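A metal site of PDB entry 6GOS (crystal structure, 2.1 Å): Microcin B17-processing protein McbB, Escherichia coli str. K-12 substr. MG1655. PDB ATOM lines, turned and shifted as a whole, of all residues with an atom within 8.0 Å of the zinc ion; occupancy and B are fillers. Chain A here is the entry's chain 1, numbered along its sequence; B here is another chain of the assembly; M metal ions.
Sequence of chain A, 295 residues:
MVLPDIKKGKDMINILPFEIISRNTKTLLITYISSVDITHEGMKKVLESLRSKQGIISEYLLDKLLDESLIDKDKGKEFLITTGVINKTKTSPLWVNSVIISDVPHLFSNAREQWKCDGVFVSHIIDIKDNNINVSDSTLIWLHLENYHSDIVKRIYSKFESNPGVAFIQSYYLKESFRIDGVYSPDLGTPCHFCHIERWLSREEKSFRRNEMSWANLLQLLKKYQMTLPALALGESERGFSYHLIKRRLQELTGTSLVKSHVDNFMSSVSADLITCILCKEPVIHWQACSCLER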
ATOM      1  N   TYR A 157       2.718   0.837  21.936  1.00  0.00           N
ATOM      2  CA  TYR A 157       2.778   0.160  20.633  1.00  0.00           C
ATOM      3  C   TYR A 157       1.505  -0.662  20.389  1.00  0.00           C
ATOM      4  O   TYR A 157       0.891  -0.606  19.327  1.00  0.00           O
ATOM      5  CB  TYR A 157       4.036  -0.727  20.572  1.00  0.00           C
ATOM      6  CG  TYR A 157       5.355  -0.003  20.306  1.00  0.00           C
ATOM      7  CD1 TYR A 157       5.444   1.402  20.198  1.00  0.00           C
ATOM      8  CD2 TYR A 157       6.538  -0.730  20.183  1.00  0.00           C
ATOM      9  CE1 TYR A 157       6.662   2.037  19.951  1.00  0.00           C
ATOM     10  CE2 TYR A 157       7.747  -0.114  19.942  1.00  0.00           C
ATOM     11  CZ  TYR A 157       7.813   1.268  19.820  1.00  0.00           C
ATOM     12  OH  TYR A 157       9.030   1.851  19.563  1.00  0.00           O
ATOM     13  N   GLU A 161       0.183   1.039  17.160  1.00  0.00           N
ATOM     14  CA  GLU A 161       0.903   0.529  15.956  1.00  0.00           C
ATOM     15  C   GLU A 161       0.040   0.443  14.696  1.00  0.00           C
ATOM     16  O   GLU A 161       0.521   0.703  13.589  1.00  0.00           O
ATOM     17  CB  GLU A 161       1.516  -0.865  16.198  1.00  0.00           C
ATOM     18  CG  GLU A 161       2.892  -0.828  16.806  1.00  0.00           C
ATOM     19  CD  GLU A 161       3.553  -2.197  16.863  1.00  0.00           C
ATOM     20  OE1 GLU A 161       2.845  -3.228  16.721  1.00  0.00           O
ATOM     21  OE2 GLU A 161       4.794  -2.224  17.039  1.00  0.00           O
ATOM     22  N   TYR A 184      10.314   5.377  14.696  1.00  0.00           N
ATOM     23  CA  TYR A 184       9.708   4.090  14.437  1.00  0.00           C
ATOM     24  C   TYR A 184       8.434   4.313  13.642  1.00  0.00           C
ATOM     25  O   TYR A 184       7.459   4.854  14.164  1.00  0.00           O
ATOM     26  CB  TYR A 184       9.378   3.375  15.766  1.00  0.00           C
ATOM     27  CG  TYR A 184       8.600   2.080  15.581  1.00  0.00           C
ATOM     28  CD1 TYR A 184       8.867   1.206  14.515  1.00  0.00           C
ATOM     29  CD2 TYR A 184       7.595   1.742  16.462  1.00  0.00           C
ATOM     30  CE1 TYR A 184       8.121   0.054  14.329  1.00  0.00           C
ATOM     31  CE2 TYR A 184       6.872   0.574  16.297  1.00  0.00           C
ATOM     32  CZ  TYR A 184       7.141  -0.267  15.245  1.00  0.00           C
ATOM     33  OH  TYR A 184       6.401  -1.400  15.106  1.00  0.00           O
ATOM     34  N   THR A 190      11.019   1.040   9.789  1.00  0.00           N
ATOM     35  CA  THR A 190      12.189   1.422  10.562  1.00  0.00           C
ATOM     36  C   THR A 190      12.220   0.762  11.948  1.00  0.00           C
ATOM     37  O   THR A 190      11.181   0.395  12.469  1.00  0.00           O
ATOM     38  CB  THR A 190      12.286   2.945  10.748  1.00  0.00           C
ATOM     39  OG1 THR A 190      11.089   3.418  11.353  1.00  0.00           O
ATOM     40  CG2 THR A 190      12.481   3.643   9.388  1.00  0.00           C
ATOM     41  N   PRO A 191      13.409   0.619  12.532  1.00  0.00           N
ATOM     42  CA  PRO A 191      13.516  -0.073  13.802  1.00  0.00           C
ATOM     43  C   PRO A 191      12.770   0.558  14.945  1.00  0.00           C
ATOM     44  O   PRO A 191      12.721   1.778  15.044  1.00  0.00           O
ATOM     45  CB  PRO A 191      15.012  -0.097  14.088  1.00  0.00           C
ATOM     46  CG  PRO A 191      15.666   0.030  12.759  1.00  0.00           C
ATOM     47  CD  PRO A 191      14.743   0.907  11.958  1.00  0.00           C
ATOM     48  N   CYS A 192      12.230  -0.298  15.815  1.00  0.00           N
ATOM     49  CA  CYS A 192      11.431   0.157  16.948  1.00  0.00           C
ATOM     50  C   CYS A 192      12.301   0.498  18.157  1.00  0.00           C
ATOM     51  O   CYS A 192      13.511   0.424  18.089  1.00  0.00           O
ATOM     52  CB  CYS A 192      10.389  -0.915  17.297  1.00  0.00           C
ATOM     53  SG  CYS A 192      11.020  -2.306  18.245  1.00  0.00           S
ATOM     54  N   HIS A 193      11.678   0.917  19.253  1.00  0.00           N
ATOM     55  CA  HIS A 193      12.362   1.155  20.516  1.00  0.00           C
ATOM     56  C   HIS A 193      13.198  -0.022  20.976  1.00  0.00           C
ATOM     57  O   HIS A 193      14.309   0.153  21.468  1.00  0.00           O
ATOM     58  CB  HIS A 193      11.367   1.443  21.634  1.00  0.00           C
ATOM     59  CG  HIS A 193      11.969   1.405  23.002  1.00  0.00           C
ATOM     60  ND1 HIS A 193      12.874   2.341  23.435  1.00  0.00           N
ATOM     61  CD2 HIS A 193      11.809   0.519  24.014  1.00  0.00           C
ATOM     62  CE1 HIS A 193      13.235   2.053  24.676  1.00  0.00           C
ATOM     63  NE2 HIS A 193      12.620   0.949  25.049  1.00  0.00           N
ATOM     64  N   PHE A 194      12.642  -1.219  20.867  1.00  0.00           N
ATOM     65  CA  PHE A 194      13.355  -2.383  21.401  1.00  0.00           C
ATOM     66  C   PHE A 194      14.588  -2.694  20.576  1.00  0.00           C
ATOM     67  O   PHE A 194      15.584  -3.164  21.105  1.00  0.00           O
ATOM     68  CB  PHE A 194      12.395  -3.583  21.611  1.00  0.00           C
ATOM     69  CG  PHE A 194      11.385  -3.322  22.695  1.00  0.00           C
ATOM     70  CD1 PHE A 194      11.781  -3.329  24.022  1.00  0.00           C
ATOM     71  CD2 PHE A 194      10.074  -2.913  22.393  1.00  0.00           C
ATOM     72  CE1 PHE A 194      10.875  -3.019  25.042  1.00  0.00           C
ATOM     73  CE2 PHE A 194       9.155  -2.616  23.397  1.00  0.00           C
ATOM     74  CZ  PHE A 194       9.560  -2.654  24.717  1.00  0.00           C
ATOM     75  N   CYS A 195      14.566  -2.348  19.301  1.00  0.00           N
ATOM     76  CA  CYS A 195      15.741  -2.488  18.470  1.00  0.00           C
ATOM     77  C   CYS A 195      16.846  -1.557  18.971  1.00  0.00           C
ATOM     78  O   CYS A 195      18.024  -1.911  18.931  1.00  0.00           O
ATOM     79  CB  CYS A 195      15.413  -2.191  17.008  1.00  0.00           C
ATOM     80  SG  CYS A 195      14.401  -3.442  16.156  1.00  0.00           S
ATOM     81  N   HIS A 196      16.463  -0.383  19.481  1.00  0.00           N
ATOM     82  CA  HIS A 196      17.410   0.581  20.006  1.00  0.00           C
ATOM     83  C   HIS A 196      17.973   0.181  21.346  1.00  0.00           C
ATOM     84  O   HIS A 196      19.211   0.160  21.500  1.00  0.00           O
ATOM     85  CB  HIS A 196      16.828   1.978  20.098  1.00  0.00           C
ATOM     86  CG  HIS A 196      16.682   2.627  18.759  1.00  0.00           C
ATOM     87  ND1 HIS A 196      15.690   2.275  17.875  1.00  0.00           N
ATOM     88  CD2 HIS A 196      17.426   3.574  18.143  1.00  0.00           C
ATOM     89  CE1 HIS A 196      15.818   3.004  16.785  1.00  0.00           C
ATOM     90  NE2 HIS A 196      16.883   3.780  16.910  1.00  0.00           N
ATOM     91  N   GLU A 198      18.209  -2.557  22.933  1.00  0.00           N
ATOM     92  CA  GLU A 198      19.096  -3.699  22.835  1.00  0.00           C
ATOM     93  C   GLU A 198      20.453  -3.307  22.269  1.00  0.00           C
ATOM     94  O   GLU A 198      21.434  -3.775  22.758  1.00  0.00           O
ATOM     95  CB  GLU A 198      18.444  -4.817  22.025  1.00  0.00           C
ATOM     96  CG  GLU A 198      17.226  -5.390  22.753  1.00  0.00           C
ATOM     97  CD  GLU A 198      17.577  -6.221  23.977  1.00  0.00           C
ATOM     98  OE1 GLU A 198      18.597  -6.965  23.929  1.00  0.00           O
ATOM     99  OE2 GLU A 198      16.837  -6.145  24.990  1.00  0.00           O
ATOM    100  N   ILE A 285      20.397  -0.826  13.555  1.00  0.00           N
ATOM    101  CA  ILE A 285      19.813  -1.932  12.806  1.00  0.00           C
ATOM    102  C   ILE A 285      18.616  -2.533  13.546  1.00  0.00           C
ATOM    103  O   ILE A 285      18.446  -2.324  14.749  1.00  0.00           O
ATOM    104  CB  ILE A 285      20.842  -3.029  12.456  1.00  0.00           C
ATOM    105  CG1 ILE A 285      21.461  -3.688  13.716  1.00  0.00           C
ATOM    106  CG2 ILE A 285      21.915  -2.474  11.535  1.00  0.00           C
ATOM    107  CD1 ILE A 285      22.270  -4.923  13.400  1.00  0.00           C
ATOM    108  N   HIS A 286      17.776  -3.244  12.795  1.00  0.00           N
ATOM    109  CA  HIS A 286      16.770  -4.124  13.401  1.00  0.00           C
ATOM    110  C   HIS A 286      17.482  -5.190  14.234  1.00  0.00           C
ATOM    111  O   HIS A 286      18.367  -5.878  13.742  1.00  0.00           O
ATOM    112  CB  HIS A 286      15.899  -4.808  12.319  1.00  0.00           C
ATOM    113  CG  HIS A 286      15.005  -3.859  11.572  1.00  0.00           C
ATOM    114  ND1 HIS A 286      15.389  -3.271  10.373  1.00  0.00           N
ATOM    115  CD2 HIS A 286      13.791  -3.353  11.875  1.00  0.00           C
ATOM    116  CE1 HIS A 286      14.423  -2.463   9.960  1.00  0.00           C
ATOM    117  NE2 HIS A 286      13.445  -2.494  10.850  1.00  0.00           N
ATOM    118  N   TRP A 287      17.124  -5.275  15.507  1.00  0.00           N
ATOM    119  CA  TRP A 287      17.549  -6.336  16.377  1.00  0.00           C
ATOM    120  C   TRP A 287      16.998  -7.690  15.928  1.00  0.00           C
ATOM    121  O   TRP A 287      15.821  -7.857  15.638  1.00  0.00           O
ATOM    122  CB  TRP A 287      17.125  -6.046  17.801  1.00  0.00           C
ATOM    123  CG  TRP A 287      17.606  -7.043  18.795  1.00  0.00           C
ATOM    124  CD1 TRP A 287      18.834  -7.602  18.849  1.00  0.00           C
ATOM    125  CD2 TRP A 287      16.858  -7.591  19.899  1.00  0.00           C
ATOM    126  NE1 TRP A 287      18.924  -8.454  19.926  1.00  0.00           N
ATOM    127  CE2 TRP A 287      17.726  -8.460  20.582  1.00  0.00           C
ATOM    128  CE3 TRP A 287      15.562  -7.385  20.393  1.00  0.00           C
ATOM    129  CZ2 TRP A 287      17.322  -9.161  21.723  1.00  0.00           C
ATOM    130  CZ3 TRP A 287      15.160  -8.093  21.546  1.00  0.00           C
ATOM    131  CH2 TRP A 287      16.044  -8.969  22.198  1.00  0.00           C
ATOM    132  N   GLN A 288      17.902  -8.673  15.859  1.00  0.00           N
ATOM    133  CA  GLN A 288      17.565  -9.969  15.331  1.00  0.00           C
ATOM    134  C   GLN A 288      16.384 -10.635  16.051  1.00  0.00           C
ATOM    135  O   GLN A 288      15.566 -11.308  15.392  1.00  0.00           O
ATOM    136  CB  GLN A 288      18.805 -10.873  15.287  1.00  0.00           C
ATOM    137  CG  GLN A 288      19.452 -11.198  16.642  1.00  0.00           C
ATOM    138  CD  GLN A 288      20.877 -11.712  16.499  1.00  0.00           C
ATOM    139  OE1 GLN A 288      21.274 -12.305  15.465  1.00  0.00           O
ATOM    140  NE2 GLN A 288      21.673 -11.459  17.519  1.00  0.00           N
ATOM    141  N   ALA A 289      16.289 -10.453  17.373  1.00  0.00           N
ATOM    142  CA  ALA A 289      15.290 -11.132  18.175  1.00  0.00           C
ATOM    143  C   ALA A 289      14.006 -10.322  18.366  1.00  0.00           C
ATOM    144  O   ALA A 289      13.160 -10.728  19.158  1.00  0.00           O
ATOM    145  CB  ALA A 289      15.864 -11.531  19.523  1.00  0.00           C
ATOM    146  N   CYS A 290      13.875  -9.196  17.663  1.00  0.00           N
ATOM    147  CA  CYS A 290      12.708  -8.336  17.737  1.00  0.00           C
ATOM    148  C   CYS A 290      11.795  -8.685  16.597  1.00  0.00           C
ATOM    149  O   CYS A 290      12.259  -8.925  15.486  1.00  0.00           O
ATOM    150  CB  CYS A 290      13.093  -6.858  17.567  1.00  0.00           C
ATOM    151  SG  CYS A 290      11.806  -5.683  18.017  1.00  0.00           S
ATOM    152  N   SER A 291      10.506  -8.609  16.838  1.00  0.00           N
ATOM    153  CA  SER A 291       9.526  -8.899  15.797  1.00  0.00           C
ATOM    154  C   SER A 291       8.779  -7.665  15.305  1.00  0.00           C
ATOM    155  O   SER A 291       7.729  -7.797  14.663  1.00  0.00           O
ATOM    156  CB  SER A 291       8.549  -9.934  16.337  1.00  0.00           C
ATOM    157  OG  SER A 291       8.012  -9.411  17.546  1.00  0.00           O
ATOM    158  N   CYS A 292       9.327  -6.459  15.516  1.00  0.00           N
ATOM    159  CA  CYS A 292       8.667  -5.261  14.999  1.00  0.00           C
ATOM    160  C   CYS A 292       8.429  -5.307  13.498  1.00  0.00           C
ATOM    161  O   CYS A 292       7.401  -4.875  13.032  1.00  0.00           O
ATOM    162  CB  CYS A 292       9.370  -3.949  15.385  1.00  0.00           C
ATOM    163  SG  CYS A 292      11.091  -3.691  14.849  1.00  0.00           S
ATOM    164  N   LEU A 293       9.363  -5.854  12.726  1.00  0.00           N
ATOM    165  CA  LEU A 293       9.194  -5.858  11.280  1.00  0.00           C
ATOM    166  C   LEU A 293       8.287  -7.011  10.777  1.00  0.00           C
ATOM    167  O   LEU A 293       7.927  -7.059   9.590  1.00  0.00           O
ATOM    168  CB  LEU A 293      10.558  -5.799  10.572  1.00  0.00           C
ATOM    169  CG  LEU A 293      11.498  -7.006  10.665  1.00  0.00           C
ATOM    170  CD1 LEU A 293      11.105  -8.088   9.661  1.00  0.00           C
ATOM    171  CD2 LEU A 293      12.927  -6.541  10.425  1.00  0.00           C
ATOM    172  N   GLU A 294       7.931  -7.931  11.677  1.00  0.00           N
ATOM    173  CA  GLU A 294       6.961  -8.985  11.377  1.00  0.00           C
ATOM    174  C   GLU A 294       5.525  -8.480  11.524  1.00  0.00           C
ATOM    175  O   GLU A 294       4.628  -9.058  10.939  1.00  0.00           O
ATOM    176  CB  GLU A 294       7.185 -10.204  12.282  1.00  0.00           C
ATOM    177  CG  GLU A 294       8.574 -10.793  12.178  1.00  0.00           C
ATOM    178  CD  GLU A 294       8.694 -12.164  12.828  1.00  0.00           C
ATOM    179  OE1 GLU A 294       8.368 -12.311  14.037  1.00  0.00           O
ATOM    180  OE2 GLU A 294       9.127 -13.110  12.124  1.00  0.00           O
ATOM    181  N   ARG A 295       5.304  -7.428  12.293  1.00  0.00           N
ATOM    182  CA  ARG A 295       3.940  -6.927  12.524  1.00  0.00           C
ATOM    183  C   ARG A 295       3.401  -6.206  11.263  1.00  0.00           C
ATOM    184  O   ARG A 295       4.145  -5.799  10.381  1.00  0.00           O
ATOM    185  CB  ARG A 295       3.864  -6.104  13.842  1.00  0.00           C
ATOM    186  CG  ARG A 295       4.079  -7.043  15.043  1.00  0.00           C
ATOM    187  CD  ARG A 295       3.601  -6.561  16.407  1.00  0.00           C
ATOM    188  NE  ARG A 295       4.375  -5.421  16.899  1.00  0.00           N
ATOM    189  CZ  ARG A 295       5.608  -5.464  17.418  1.00  0.00           C
ATOM    190  NH1 ARG A 295       6.255  -6.619  17.579  1.00  0.00           N
ATOM    191  NH2 ARG A 295       6.208  -4.325  17.809  1.00  0.00           N
ATOM    192  OXT ARG A 295       2.196  -6.126  11.041  1.00  0.00           O
ATOM    193  N   ARG B 252      16.209  -8.084   8.396  1.00  0.00           N
ATOM    194  CA  ARG B 252      17.244  -8.842   9.119  1.00  0.00           C
ATOM    195  C   ARG B 252      18.096  -9.751   8.222  1.00  0.00           C
ATOM    196  O   ARG B 252      19.250 -10.017   8.537  1.00  0.00           O
ATOM    197  CB  ARG B 252      16.621  -9.602  10.279  1.00  0.00           C
ATOM    198  CG  ARG B 252      16.041  -8.670  11.343  1.00  0.00           C
ATOM    199  CD  ARG B 252      15.081  -9.361  12.296  1.00  0.00           C
ATOM    200  NE  ARG B 252      13.985 -10.015  11.587  1.00  0.00           N
ATOM    201  CZ  ARG B 252      13.085 -10.822  12.145  1.00  0.00           C
ATOM    202  NH1 ARG B 252      13.081 -11.062  13.443  1.00  0.00           N
ATOM    203  NH2 ARG B 252      12.145 -11.383  11.387  1.00  0.00           N
HETATM  204 ZN    ZN M   1      12.229  -3.700  16.872  1.00  0.00          ZN
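O of Cys 290 sits at hydrogen-bond distance from NH1 of Arg 252 of chain B (3.1 Å). The backbone carbonyl oxygen (O) of Cys 192 is in hydrogen-bond range of a ring nitrogen (ND1) of His 196 (2.9 Å). The backbone NH of Phe 194 sits close to the side-chain sulfur of Cys 192 (3.3 Å). SG of Cys 195 lies close to N of Trp 287 (3.3 Å).
The zinc ion is bound by the side-chain sulfur of Cys 192 (2.3 Å), the side-chain sulfur of Cys 195 (2.3 Å), the side-chain sulfur of Cys 292 (2.3 Å) and the side-chain sulfur of Cys 290 (2.3 Å).
Along chain A the residues within 4 Å of the zinc ion span positions 192 to 292.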
